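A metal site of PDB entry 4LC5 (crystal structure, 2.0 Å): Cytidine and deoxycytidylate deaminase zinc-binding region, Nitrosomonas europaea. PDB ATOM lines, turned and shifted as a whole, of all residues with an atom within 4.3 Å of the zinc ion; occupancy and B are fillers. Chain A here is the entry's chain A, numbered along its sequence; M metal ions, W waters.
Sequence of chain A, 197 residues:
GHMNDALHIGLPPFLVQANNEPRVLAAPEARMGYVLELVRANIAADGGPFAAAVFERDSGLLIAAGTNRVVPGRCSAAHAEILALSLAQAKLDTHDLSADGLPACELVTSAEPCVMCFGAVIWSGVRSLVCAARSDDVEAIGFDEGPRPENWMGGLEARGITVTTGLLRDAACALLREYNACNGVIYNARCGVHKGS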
ATOM      1  N   HIS A  79     -24.706  31.633 -16.326  1.00  0.00           N
ATOM      2  CA  HIS A  79     -25.870  30.953 -16.860  1.00  0.00           C
ATOM      3  C   HIS A  79     -26.748  30.547 -15.678  1.00  0.00           C
ATOM      4  O   HIS A  79     -26.290  30.528 -14.556  1.00  0.00           O
ATOM      5  CB  HIS A  79     -25.423  29.705 -17.589  1.00  0.00           C
ATOM      6  CG  HIS A  79     -24.851  29.953 -18.926  1.00  0.00           C
ATOM      7  ND1 HIS A  79     -24.847  29.029 -19.875  1.00  0.00           N
ATOM      8  CD2 HIS A  79     -24.293  31.112 -19.511  1.00  0.00           C
ATOM      9  CE1 HIS A  79     -24.235  29.484 -21.025  1.00  0.00           C
ATOM     10  NE2 HIS A  79     -23.934  30.779 -20.824  1.00  0.00           N
ATOM     11  N   GLU A  81     -27.955  27.842 -14.575  1.00  0.00           N
ATOM     12  CA  GLU A  81     -27.660  26.630 -13.885  1.00  0.00           C
ATOM     13  C   GLU A  81     -26.462  26.844 -12.927  1.00  0.00           C
ATOM     14  O   GLU A  81     -26.497  26.389 -11.779  1.00  0.00           O
ATOM     15  CB  GLU A  81     -27.355  25.488 -14.865  1.00  0.00           C
ATOM     16  CG  GLU A  81     -28.499  25.185 -15.790  1.00  0.00           C
ATOM     17  CD  GLU A  81     -28.336  25.962 -17.129  1.00  0.00           C
ATOM     18  OE1 GLU A  81     -28.187  27.178 -17.137  1.00  0.00           O
ATOM     19  OE2 GLU A  81     -28.267  25.295 -18.186  1.00  0.00           O
ATOM     20  N   CYS A 114     -26.143  23.840 -21.771  1.00  0.00           N
ATOM     21  CA  CYS A 114     -24.958  24.027 -22.688  1.00  0.00           C
ATOM     22  C   CYS A 114     -23.766  23.226 -22.159  1.00  0.00           C
ATOM     23  O   CYS A 114     -23.819  22.602 -21.059  1.00  0.00           O
ATOM     24  CB  CYS A 114     -24.648  25.536 -22.833  1.00  0.00           C
ATOM     25  SG  CYS A 114     -23.624  26.110 -21.457  1.00  0.00           S
ATOM     26  N   MET A 116     -20.859  23.938 -21.030  1.00  0.00           N
ATOM     27  CA  MET A 116     -20.417  24.458 -19.700  1.00  0.00           C
ATOM     28  C   MET A 116     -21.285  23.964 -18.533  1.00  0.00           C
ATOM     29  O   MET A 116     -20.759  23.474 -17.548  1.00  0.00           O
ATOM     30  CB  MET A 116     -20.406  25.985 -19.672  1.00  0.00           C
ATOM     31  CG  MET A 116     -19.914  26.604 -18.311  1.00  0.00           C
ATOM     32  SD  MET A 116     -19.814  28.430 -18.346  1.00  0.00           S
ATOM     33  CE  MET A 116     -21.521  28.981 -18.455  1.00  0.00           C
ATOM     34  N   CYS A 117     -22.607  24.152 -18.649  1.00  0.00           N
ATOM     35  CA  CYS A 117     -23.548  23.825 -17.572  1.00  0.00           C
ATOM     36  C   CYS A 117     -23.683  22.319 -17.373  1.00  0.00           C
ATOM     37  O   CYS A 117     -23.808  21.869 -16.229  1.00  0.00           O
ATOM     38  CB  CYS A 117     -24.907  24.545 -17.807  1.00  0.00           C
ATOM     39  SG  CYS A 117     -24.627  26.320 -17.571  1.00  0.00           S
HETATM   40 ZN    ZN M   1     -24.918  26.936 -19.747  1.00  0.00          ZN
HETATM   41  O   HOH W   1     -26.786  26.109 -20.275  1.00  0.00           O
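Of the 5 residues printed, 3 come within 4 Å of the zinc ion.
SG of Cys 114 lies close to N of Met 116, 3.5 Å away.
The side-chain sulfur (SG) of Cys 117 lies close to the side-chain carboxylate (OE1) of Glu 81, at 3.7 Å.
Water W1 bridges OE2 of Glu 81 and N of Cys 114.
The zinc ion is bound by ND1 of His 79 (2.1 Å), water W1 (2.1 Å), SG of Cys 117 (2.3 Å) and SG of Cys 114 (2.3 Å).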
